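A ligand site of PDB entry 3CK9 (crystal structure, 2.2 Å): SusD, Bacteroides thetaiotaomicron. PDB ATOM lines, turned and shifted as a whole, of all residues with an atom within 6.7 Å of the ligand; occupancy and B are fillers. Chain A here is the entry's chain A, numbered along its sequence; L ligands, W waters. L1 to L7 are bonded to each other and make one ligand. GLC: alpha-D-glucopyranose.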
ATOM      1  N   GLN A  48      -1.014 -20.501  -4.018  1.00  0.00           N
ATOM      2  CA  GLN A  48      -2.050 -21.425  -3.561  1.00  0.00           C
ATOM      3  C   GLN A  48      -1.779 -22.851  -4.003  1.00  0.00           C
ATOM      4  O   GLN A  48      -1.756 -23.149  -5.202  1.00  0.00           O
ATOM      5  CB  GLN A  48      -3.425 -21.003  -4.101  1.00  0.00           C
ATOM      6  CG  GLN A  48      -4.532 -22.037  -3.856  1.00  0.00           C
ATOM      7  CD  GLN A  48      -5.801 -21.743  -4.642  1.00  0.00           C
ATOM      8  OE1 GLN A  48      -5.745 -21.674  -5.879  1.00  0.00           O
ATOM      9  NE2 GLN A  48      -6.865 -21.576  -4.001  1.00  0.00           N
ATOM     10  N   ASP A  49      -1.585 -23.740  -3.027  1.00  0.00           N
ATOM     11  CA  ASP A  49      -1.358 -25.140  -3.321  1.00  0.00           C
ATOM     12  C   ASP A  49      -2.610 -25.642  -4.038  1.00  0.00           C
ATOM     13  O   ASP A  49      -3.730 -25.242  -3.696  1.00  0.00           O
ATOM     14  CB  ASP A  49      -1.153 -25.937  -2.020  1.00  0.00           C
ATOM     15  CG  ASP A  49       0.285 -25.918  -1.532  1.00  0.00           C
ATOM     16  OD1 ASP A  49       0.547 -26.434  -0.417  1.00  0.00           O
ATOM     17  OD2 ASP A  49       1.156 -25.397  -2.254  1.00  0.00           O
ATOM     18  N   GLU A  50      -2.430 -26.494  -5.040  1.00  0.00           N
ATOM     19  CA  GLU A  50      -3.560 -27.023  -5.788  1.00  0.00           C
ATOM     20  C   GLU A  50      -4.561 -27.679  -4.851  1.00  0.00           C
ATOM     21  O   GLU A  50      -5.785 -27.579  -5.055  1.00  0.00           O
ATOM     22  CB  GLU A  50      -3.090 -28.055  -6.824  1.00  0.00           C
ATOM     23  CG  GLU A  50      -4.214 -28.629  -7.676  1.00  0.00           C
ATOM     24  CD  GLU A  50      -3.732 -29.726  -8.621  1.00  0.00           C
ATOM     25  OE1 GLU A  50      -2.820 -29.457  -9.421  1.00  0.00           O
ATOM     26  OE2 GLU A  50      -4.266 -30.845  -8.546  1.00  0.00           O
ATOM     27  N   GLY A  51      -4.049 -28.346  -3.825  1.00  0.00           N
ATOM     28  CA  GLY A  51      -4.899 -29.030  -2.859  1.00  0.00           C
ATOM     29  C   GLY A  51      -5.739 -28.135  -1.978  1.00  0.00           C
ATOM     30  O   GLY A  51      -6.516 -28.623  -1.163  1.00  0.00           O
ATOM     31  N   GLU A  52      -5.579 -26.821  -2.140  1.00  0.00           N
ATOM     32  CA  GLU A  52      -6.326 -25.832  -1.362  1.00  0.00           C
ATOM     33  C   GLU A  52      -7.442 -25.213  -2.189  1.00  0.00           C
ATOM     34  O   GLU A  52      -8.272 -24.457  -1.668  1.00  0.00           O
ATOM     35  CB  GLU A  52      -5.392 -24.696  -0.911  1.00  0.00           C
ATOM     36  CG  GLU A  52      -4.262 -25.087   0.030  1.00  0.00           C
ATOM     37  CD  GLU A  52      -4.619 -24.906   1.499  1.00  0.00           C
ATOM     38  OE1 GLU A  52      -3.752 -25.152   2.354  1.00  0.00           O
ATOM     39  OE2 GLU A  52      -5.760 -24.506   1.794  1.00  0.00           O
ATOM     40  N   ARG A  57     -12.952 -28.289   0.259  1.00  0.00           N
ATOM     41  CA  ARG A  57     -12.078 -27.718   1.276  1.00  0.00           C
ATOM     42  C   ARG A  57     -12.281 -26.236   1.560  1.00  0.00           C
ATOM     43  O   ARG A  57     -12.332 -25.824   2.728  1.00  0.00           O
ATOM     44  CB  ARG A  57     -10.617 -27.981   0.882  1.00  0.00           C
ATOM     45  CG  ARG A  57      -9.611 -27.514   1.907  1.00  0.00           C
ATOM     46  CD  ARG A  57      -8.232 -27.943   1.497  1.00  0.00           C
ATOM     47  NE  ARG A  57      -7.245 -27.581   2.509  1.00  0.00           N
ATOM     48  CZ  ARG A  57      -6.011 -28.052   2.535  1.00  0.00           C
ATOM     49  NH1 ARG A  57      -5.616 -28.898   1.595  1.00  0.00           N
ATOM     50  NH2 ARG A  57      -5.169 -27.684   3.496  1.00  0.00           N
ATOM     51  N   TRP A  72      -7.390 -25.289  13.451  1.00  0.00           N
ATOM     52  CA  TRP A  72      -6.341 -25.705  12.537  1.00  0.00           C
ATOM     53  C   TRP A  72      -5.045 -25.555  13.350  1.00  0.00           C
ATOM     54  O   TRP A  72      -4.696 -24.452  13.769  1.00  0.00           O
ATOM     55  CB  TRP A  72      -6.319 -24.816  11.289  1.00  0.00           C
ATOM     56  CG  TRP A  72      -5.326 -25.254  10.256  1.00  0.00           C
ATOM     57  CD1 TRP A  72      -4.057 -24.789  10.099  1.00  0.00           C
ATOM     58  CD2 TRP A  72      -5.491 -26.298   9.288  1.00  0.00           C
ATOM     59  NE1 TRP A  72      -3.414 -25.480   9.088  1.00  0.00           N
ATOM     60  CE2 TRP A  72      -4.284 -26.407   8.573  1.00  0.00           C
ATOM     61  CE3 TRP A  72      -6.558 -27.151   8.949  1.00  0.00           C
ATOM     62  CZ2 TRP A  72      -4.095 -27.338   7.540  1.00  0.00           C
ATOM     63  CZ3 TRP A  72      -6.374 -28.074   7.920  1.00  0.00           C
ATOM     64  CH2 TRP A  72      -5.150 -28.161   7.230  1.00  0.00           C
ATOM     65  N   TRP A  74      -1.775 -25.814  12.557  1.00  0.00           N
ATOM     66  CA  TRP A  74      -0.655 -25.051  12.017  1.00  0.00           C
ATOM     67  C   TRP A  74      -1.051 -23.633  11.637  1.00  0.00           C
ATOM     68  O   TRP A  74      -1.309 -23.330  10.474  1.00  0.00           O
ATOM     69  CB  TRP A  74      -0.052 -25.809  10.819  1.00  0.00           C
ATOM     70  CG  TRP A  74       0.291 -27.220  11.177  1.00  0.00           C
ATOM     71  CD1 TRP A  74      -0.527 -28.310  11.067  1.00  0.00           C
ATOM     72  CD2 TRP A  74       1.507 -27.694  11.759  1.00  0.00           C
ATOM     73  NE1 TRP A  74       0.103 -29.431  11.555  1.00  0.00           N
ATOM     74  CE2 TRP A  74       1.347 -29.079  11.985  1.00  0.00           C
ATOM     75  CE3 TRP A  74       2.713 -27.078  12.125  1.00  0.00           C
ATOM     76  CZ2 TRP A  74       2.363 -29.865  12.555  1.00  0.00           C
ATOM     77  CZ3 TRP A  74       3.715 -27.860  12.696  1.00  0.00           C
ATOM     78  CH2 TRP A  74       3.534 -29.235  12.904  1.00  0.00           C
ATOM     79  N   LYS A  76       0.649 -21.037  11.312  1.00  0.00           N
ATOM     80  CA  LYS A  76       1.549 -20.296  10.438  1.00  0.00           C
ATOM     81  C   LYS A  76       1.073 -20.341   8.991  1.00  0.00           C
ATOM     82  O   LYS A  76       1.505 -19.542   8.165  1.00  0.00           O
ATOM     83  CB  LYS A  76       2.982 -20.845  10.548  1.00  0.00           C
ATOM     84  CG  LYS A  76       3.612 -20.660  11.920  1.00  0.00           C
ATOM     85  CD  LYS A  76       5.051 -21.136  11.944  1.00  0.00           C
ATOM     86  CE  LYS A  76       5.631 -21.101  13.357  1.00  0.00           C
ATOM     87  NZ  LYS A  76       5.526 -19.747  13.953  1.00  0.00           N
ATOM     88  N   ASN A  77       0.184 -21.274   8.666  1.00  0.00           N
ATOM     89  CA  ASN A  77      -0.347 -21.359   7.308  1.00  0.00           C
ATOM     90  C   ASN A  77      -1.053 -20.040   7.015  1.00  0.00           C
ATOM     91  O   ASN A  77      -1.747 -19.487   7.866  1.00  0.00           O
ATOM     92  CB  ASN A  77      -1.348 -22.508   7.178  1.00  0.00           C
ATOM     93  CG  ASN A  77      -0.693 -23.870   7.250  1.00  0.00           C
ATOM     94  OD1 ASN A  77      -1.369 -24.890   7.165  1.00  0.00           O
ATOM     95  ND2 ASN A  77       0.629 -23.897   7.398  1.00  0.00           N
ATOM     96  N   ARG A  94      -7.995 -17.079   1.636  1.00  0.00           N
ATOM     97  CA  ARG A  94      -8.930 -18.193   1.688  1.00  0.00           C
ATOM     98  C   ARG A  94     -10.350 -17.794   1.292  1.00  0.00           C
ATOM     99  O   ARG A  94     -11.171 -18.645   0.959  1.00  0.00           O
ATOM    100  CB  ARG A  94      -8.904 -18.843   3.069  1.00  0.00           C
ATOM    101  CG  ARG A  94      -7.529 -19.404   3.431  1.00  0.00           C
ATOM    102  CD  ARG A  94      -7.496 -20.116   4.767  1.00  0.00           C
ATOM    103  NE  ARG A  94      -6.161 -20.618   5.067  1.00  0.00           N
ATOM    104  CZ  ARG A  94      -5.640 -21.727   4.540  1.00  0.00           C
ATOM    105  NH1 ARG A  94      -6.346 -22.469   3.702  1.00  0.00           N
ATOM    106  NH2 ARG A  94      -4.389 -22.089   4.843  1.00  0.00           N
ATOM    107  N   TYR A 272      -6.718 -33.716  -1.994  1.00  0.00           N
ATOM    108  CA  TYR A 272      -6.173 -33.369  -0.687  1.00  0.00           C
ATOM    109  C   TYR A 272      -7.231 -32.665   0.145  1.00  0.00           C
ATOM    110  O   TYR A 272      -7.230 -32.763   1.381  1.00  0.00           O
ATOM    111  CB  TYR A 272      -4.953 -32.444  -0.813  1.00  0.00           C
ATOM    112  CG  TYR A 272      -3.715 -33.130  -1.327  1.00  0.00           C
ATOM    113  CD1 TYR A 272      -3.339 -33.027  -2.662  1.00  0.00           C
ATOM    114  CD2 TYR A 272      -2.916 -33.891  -0.483  1.00  0.00           C
ATOM    115  CE1 TYR A 272      -2.196 -33.645  -3.145  1.00  0.00           C
ATOM    116  CE2 TYR A 272      -1.760 -34.523  -0.950  1.00  0.00           C
ATOM    117  CZ  TYR A 272      -1.407 -34.396  -2.285  1.00  0.00           C
ATOM    118  OH  TYR A 272      -0.260 -34.987  -2.741  1.00  0.00           O
ATOM    119  N   GLY A 273      -8.148 -31.981  -0.532  1.00  0.00           N
ATOM    120  CA  GLY A 273      -9.208 -31.282   0.160  1.00  0.00           C
ATOM    121  C   GLY A 273     -10.502 -32.064   0.143  1.00  0.00           C
ATOM    122  O   GLY A 273     -11.581 -31.501   0.337  1.00  0.00           O
ATOM    123  N   TYR A 277      -8.660 -34.977   3.323  1.00  0.00           N
ATOM    124  CA  TYR A 277      -8.600 -33.852   4.261  1.00  0.00           C
ATOM    125  C   TYR A 277      -9.225 -34.195   5.609  1.00  0.00           C
ATOM    126  O   TYR A 277      -8.684 -33.869   6.654  1.00  0.00           O
ATOM    127  CB  TYR A 277      -9.352 -32.675   3.647  1.00  0.00           C
ATOM    128  CG  TYR A 277      -9.214 -31.360   4.351  1.00  0.00           C
ATOM    129  CD1 TYR A 277      -7.976 -30.729   4.476  1.00  0.00           C
ATOM    130  CD2 TYR A 277     -10.344 -30.702   4.845  1.00  0.00           C
ATOM    131  CE1 TYR A 277      -7.872 -29.461   5.061  1.00  0.00           C
ATOM    132  CE2 TYR A 277     -10.249 -29.443   5.436  1.00  0.00           C
ATOM    133  CZ  TYR A 277      -9.015 -28.838   5.535  1.00  0.00           C
ATOM    134  OH  TYR A 277      -8.919 -27.594   6.106  1.00  0.00           O
ATOM    135  N   ASN A 294      -0.473 -41.344   6.486  1.00  0.00           N
ATOM    136  CA  ASN A 294      -0.126 -39.954   6.685  1.00  0.00           C
ATOM    137  C   ASN A 294      -1.080 -39.174   7.587  1.00  0.00           C
ATOM    138  O   ASN A 294      -2.226 -38.910   7.226  1.00  0.00           O
ATOM    139  CB  ASN A 294      -0.037 -39.269   5.319  1.00  0.00           C
ATOM    140  CG  ASN A 294       1.218 -38.436   5.167  1.00  0.00           C
ATOM    141  OD1 ASN A 294       2.338 -38.971   5.139  1.00  0.00           O
ATOM    142  ND2 ASN A 294       1.058 -37.119   5.055  1.00  0.00           N
ATOM    143  N   GLY A 295      -0.595 -38.813   8.773  1.00  0.00           N
ATOM    144  CA  GLY A 295      -1.385 -38.036   9.696  1.00  0.00           C
ATOM    145  C   GLY A 295      -0.849 -36.623   9.645  1.00  0.00           C
ATOM    146  O   GLY A 295       0.293 -36.393  10.025  1.00  0.00           O
ATOM    147  N   TRP A 296      -1.648 -35.670   9.169  1.00  0.00           N
ATOM    148  CA  TRP A 296      -1.186 -34.285   9.064  1.00  0.00           C
ATOM    149  C   TRP A 296      -1.267 -33.508  10.373  1.00  0.00           C
ATOM    150  O   TRP A 296      -0.695 -32.429  10.496  1.00  0.00           O
ATOM    151  CB  TRP A 296      -2.018 -33.516   8.017  1.00  0.00           C
ATOM    152  CG  TRP A 296      -2.167 -34.187   6.682  1.00  0.00           C
ATOM    153  CD1 TRP A 296      -1.511 -35.290   6.224  1.00  0.00           C
ATOM    154  CD2 TRP A 296      -3.016 -33.755   5.610  1.00  0.00           C
ATOM    155  NE1 TRP A 296      -1.886 -35.574   4.938  1.00  0.00           N
ATOM    156  CE2 TRP A 296      -2.810 -34.642   4.534  1.00  0.00           C
ATOM    157  CE3 TRP A 296      -3.930 -32.703   5.454  1.00  0.00           C
ATOM    158  CZ2 TRP A 296      -3.485 -34.515   3.317  1.00  0.00           C
ATOM    159  CZ3 TRP A 296      -4.596 -32.573   4.240  1.00  0.00           C
ATOM    160  CH2 TRP A 296      -4.378 -33.478   3.188  1.00  0.00           C
ATOM    161  N   SER A 297      -1.999 -34.050  11.344  1.00  0.00           N
ATOM    162  CA  SER A 297      -2.179 -33.392  12.627  1.00  0.00           C
ATOM    163  C   SER A 297      -2.621 -31.929  12.451  1.00  0.00           C
ATOM    164  O   SER A 297      -2.013 -31.019  12.998  1.00  0.00           O
ATOM    165  CB  SER A 297      -0.882 -33.465  13.456  1.00  0.00           C
ATOM    166  OG  SER A 297       0.231 -32.998  12.719  1.00  0.00           O
ATOM    167  N   CYS A 298      -3.691 -31.721  11.688  1.00  0.00           N
ATOM    168  CA  CYS A 298      -4.206 -30.369  11.424  1.00  0.00           C
ATOM    169  C   CYS A 298      -5.500 -29.985  12.146  1.00  0.00           C
ATOM    170  O   CYS A 298      -5.552 -28.974  12.832  1.00  0.00           O
ATOM    171  CB  CYS A 298      -4.425 -30.162   9.926  1.00  0.00           C
ATOM    172  SG  CYS A 298      -2.923 -30.117   8.949  1.00  0.00           S
HETATM  173  C1  GLC L   1       0.753 -30.558  -3.032  1.00  0.00           C
HETATM  174  C2  GLC L   1      -0.725 -30.176  -2.790  1.00  0.00           C
HETATM  175  C3  GLC L   1      -0.881 -29.721  -1.331  1.00  0.00           C
HETATM  176  C4  GLC L   1      -0.410 -30.860  -0.394  1.00  0.00           C
HETATM  177  C5  GLC L   1       1.069 -31.181  -0.728  1.00  0.00           C
HETATM  178  C6  GLC L   1       1.569 -32.314   0.179  1.00  0.00           C
HETATM  179  O1  GLC L   1       0.898 -31.038  -4.380  1.00  0.00           O
HETATM  180  O2  GLC L   1      -1.141 -29.139  -3.688  1.00  0.00           O
HETATM  181  O3  GLC L   1      -2.236 -29.383  -1.060  1.00  0.00           O
HETATM  182  O4  GLC L   1      -0.534 -30.438   0.969  1.00  0.00           O
HETATM  183  O5  GLC L   1       1.191 -31.600  -2.124  1.00  0.00           O
HETATM  184  O6  GLC L   1       2.872 -32.726  -0.227  1.00  0.00           O
HETATM  185  C1  GLC L   2      -1.608 -31.174   1.584  1.00  0.00           C
HETATM  186  C2  GLC L   2      -2.511 -30.179   2.345  1.00  0.00           C
HETATM  187  C3  GLC L   2      -1.630 -29.430   3.346  1.00  0.00           C
HETATM  188  C4  GLC L   2      -0.980 -30.449   4.302  1.00  0.00           C
HETATM  189  C5  GLC L   2      -0.167 -31.475   3.473  1.00  0.00           C
HETATM  190  C6  GLC L   2       0.462 -32.509   4.408  1.00  0.00           C
HETATM  191  O2  GLC L   2      -3.095 -29.231   1.457  1.00  0.00           O
HETATM  192  O3  GLC L   2      -2.408 -28.479   4.090  1.00  0.00           O
HETATM  193  O4  GLC L   2      -0.117 -29.754   5.214  1.00  0.00           O
HETATM  194  O5  GLC L   2      -1.036 -32.150   2.514  1.00  0.00           O
HETATM  195  O6  GLC L   2       1.226 -33.455   3.665  1.00  0.00           O
HETATM  196  C1  GLC L   3      -0.665 -29.692   6.549  1.00  0.00           C
HETATM  197  C2  GLC L   3      -0.350 -28.301   7.157  1.00  0.00           C
HETATM  198  C3  GLC L   3       1.170 -28.118   7.170  1.00  0.00           C
HETATM  199  C4  GLC L   3       1.799 -29.242   8.010  1.00  0.00           C
HETATM  200  C5  GLC L   3       1.387 -30.626   7.377  1.00  0.00           C
HETATM  201  C6  GLC L   3       1.972 -31.789   8.194  1.00  0.00           C
HETATM  202  O2  GLC L   3      -0.933 -27.263   6.364  1.00  0.00           O
HETATM  203  O3  GLC L   3       1.519 -26.841   7.718  1.00  0.00           O
HETATM  204  O4  GLC L   3       3.228 -29.075   7.974  1.00  0.00           O
HETATM  205  O5  GLC L   3      -0.065 -30.756   7.363  1.00  0.00           O
HETATM  206  O6  GLC L   3       1.659 -31.655   9.582  1.00  0.00           O
HETATM  207  C1  GLC L   4       3.845 -29.077   9.278  1.00  0.00           C
HETATM  208  C2  GLC L   4       4.871 -27.907   9.296  1.00  0.00           C
HETATM  209  C3  GLC L   4       5.830 -28.112   8.115  1.00  0.00           C
HETATM  210  C4  GLC L   4       6.518 -29.484   8.242  1.00  0.00           C
HETATM  211  C5  GLC L   4       5.395 -30.600   8.281  1.00  0.00           C
HETATM  212  C6  GLC L   4       5.999 -31.995   8.459  1.00  0.00           C
HETATM  213  O2  GLC L   4       4.214 -26.645   9.146  1.00  0.00           O
HETATM  214  O3  GLC L   4       6.813 -27.070   8.084  1.00  0.00           O
HETATM  215  O4  GLC L   4       7.357 -29.593   7.059  1.00  0.00           O
HETATM  216  O5  GLC L   4       4.524 -30.364   9.428  1.00  0.00           O
HETATM  217  O6  GLC L   4       6.826 -32.016   9.617  1.00  0.00           O
HETATM  218  C1  GLC L   5       8.514 -30.465   7.089  1.00  0.00           C
HETATM  219  C2  GLC L   5       9.703 -29.697   6.419  1.00  0.00           C
HETATM  220  C3  GLC L   5       9.185 -29.199   5.049  1.00  0.00           C
HETATM  221  C4  GLC L   5       8.738 -30.406   4.203  1.00  0.00           C
HETATM  222  C5  GLC L   5       7.659 -31.212   4.973  1.00  0.00           C
HETATM  223  C6  GLC L   5       7.252 -32.431   4.122  1.00  0.00           C
HETATM  224  O2  GLC L   5      10.091 -28.561   7.189  1.00  0.00           O
HETATM  225  O3  GLC L   5      10.200 -28.466   4.372  1.00  0.00           O
HETATM  226  O4  GLC L   5       8.186 -29.963   2.950  1.00  0.00           O
HETATM  227  O5  GLC L   5       8.186 -31.650   6.262  1.00  0.00           O
HETATM  228  O6  GLC L   5       8.295 -33.404   4.147  1.00  0.00           O
HETATM  229  C1  GLC L   6       9.107 -30.001   1.845  1.00  0.00           C
HETATM  230  C2  GLC L   6       9.103 -28.594   1.187  1.00  0.00           C
HETATM  231  C3  GLC L   6       7.669 -28.268   0.796  1.00  0.00           C
HETATM  232  C4  GLC L   6       7.151 -29.360  -0.209  1.00  0.00           C
HETATM  233  C5  GLC L   6       7.267 -30.740   0.448  1.00  0.00           C
HETATM  234  C6  GLC L   6       6.795 -31.803  -0.561  1.00  0.00           C
HETATM  235  O2  GLC L   6       9.558 -27.605   2.098  1.00  0.00           O
HETATM  236  O3  GLC L   6       7.615 -26.952   0.211  1.00  0.00           O
HETATM  237  O4  GLC L   6       5.756 -29.169  -0.614  1.00  0.00           O
HETATM  238  O5  GLC L   6       8.642 -31.002   0.871  1.00  0.00           O
HETATM  239  O6  GLC L   6       6.622 -33.057   0.090  1.00  0.00           O
HETATM  240  C1  GLC L   7       5.476 -27.873  -1.168  1.00  0.00           C
HETATM  241  C2  GLC L   7       3.958 -27.668  -1.220  1.00  0.00           C
HETATM  242  C3  GLC L   7       3.349 -28.685  -2.178  1.00  0.00           C
HETATM  243  C4  GLC L   7       3.984 -28.494  -3.563  1.00  0.00           C
HETATM  244  C5  GLC L   7       5.511 -28.698  -3.430  1.00  0.00           C
HETATM  245  C6  GLC L   7       6.162 -28.509  -4.793  1.00  0.00           C
HETATM  246  O2  GLC L   7       3.387 -27.821   0.088  1.00  0.00           O
HETATM  247  O3  GLC L   7       1.944 -28.496  -2.243  1.00  0.00           O
HETATM  248  O4  GLC L   7       3.437 -29.445  -4.482  1.00  0.00           O
HETATM  249  O5  GLC L   7       6.071 -27.736  -2.494  1.00  0.00           O
HETATM  250  O6  GLC L   7       7.572 -28.683  -4.652  1.00  0.00           O
HETATM  251  O   HOH W   1      10.862 -33.369   4.875  1.00  0.00           O
HETATM  252  O   HOH W   2       8.620 -26.737  -2.759  1.00  0.00           O
HETATM  253  O   HOH W   3      -1.580 -26.717   1.453  1.00  0.00           O
HETATM  254  O   HOH W   4       3.754 -31.767   4.107  1.00  0.00           O
HETATM  255  O   HOH W   5       4.423 -24.300  10.439  1.00  0.00           O
HETATM  256  O   HOH W   6       0.483 -35.288   1.797  1.00  0.00           O
HETATM  257  O   HOH W   7       3.544 -32.702  11.285  1.00  0.00           O
HETATM  258  O   HOH W   8       4.148 -32.560  -2.669  1.00  0.00           O
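OD1 of Asn 77 lies within hydrogen-bond range of O2 of GLC L3, at 2.5 Å.
An oxygen (O5) of GLC L3 sits close to the side-chain sulfur (SG) of Cys 298, 3.3 Å away.
An oxygen (O2) of GLC L1 sits at hydrogen-bond distance from the backbone NH of Glu 50, at 3.2 Å.
The backbone NH (N) of Gly 51 is in hydrogen-bond range of an oxygen (O2) of GLC L1, 3.0 Å away.
NE1 of Trp 74 is in hydrogen-bond range of O6 of GLC L3, at 3.4 Å.
The backbone carbonyl oxygen of Trp 296 lies within hydrogen-bond range of an oxygen (O6) of GLC L3 (2.6 Å).
An oxygen (O2) of GLC L2 is in hydrogen-bond range of the guanidinium group (NH1) of Arg 57 (2.5 Å).
The side-chain carboxylate (OD1) of Asp 49 sits at hydrogen-bond distance from an oxygen (O3) of GLC L7.
N of Arg 57 lies within hydrogen-bond range of O of Gly 273, 3.5 Å away.
The backbone carbonyl oxygen of Tyr 272 lies close to the backbone NH of Tyr 277, at 3.3 Å.
O of Trp 296 lies within hydrogen-bond range of NE1 of Trp 74, at 3.3 Å.
The indole nitrogen (NE1) of Trp 296 lies close to the side-chain amide nitrogen (ND2) of Asn 294, at 3.3 Å.
NH2 of Arg 57 lies within salt-bridge range of OE1 of Glu 52 (3.1 Å).
O of Trp 74 sits close to NE1 of Trp 72 (3.3 Å).
The guanidinium group (NH1) of Arg 94 lies within salt-bridge range of the side-chain carboxylate (OE2) of Glu 52, 2.9 Å away.
NH1 of Arg 57 lies within hydrogen-bond range of O of Gly 51.
Glu 52 touches the ligand.
Trp 72 touches the ligand.
CD2 of Tyr 272 touches C1 of GLC L2, 3.7 Å away.
ND2 of Asn 294 touches O6 of GLC L2, at 3.9 Å.
OG of Ser 297 touches O6 of GLC L3 (3.7 Å).
Hydrophobic or aromatic side chains that line the ligand: Trp 72, Trp 74, Tyr 272 and Trp 296.
Within 4 Å of the ligand: Asp 49, Glu 50, Gly 51, Glu 52, Arg 57, Trp 72, Trp 74, Asn 77, Tyr 272, Asn 294, Trp 296, Ser 297 and Cys 298.
Water W3 lies within hydrogen-bond range of OE1 of Glu 52 (2.8 Å), OD1 of Asp 49 (2.8 Å) and O2 of GLC L2 (2.9 Å).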
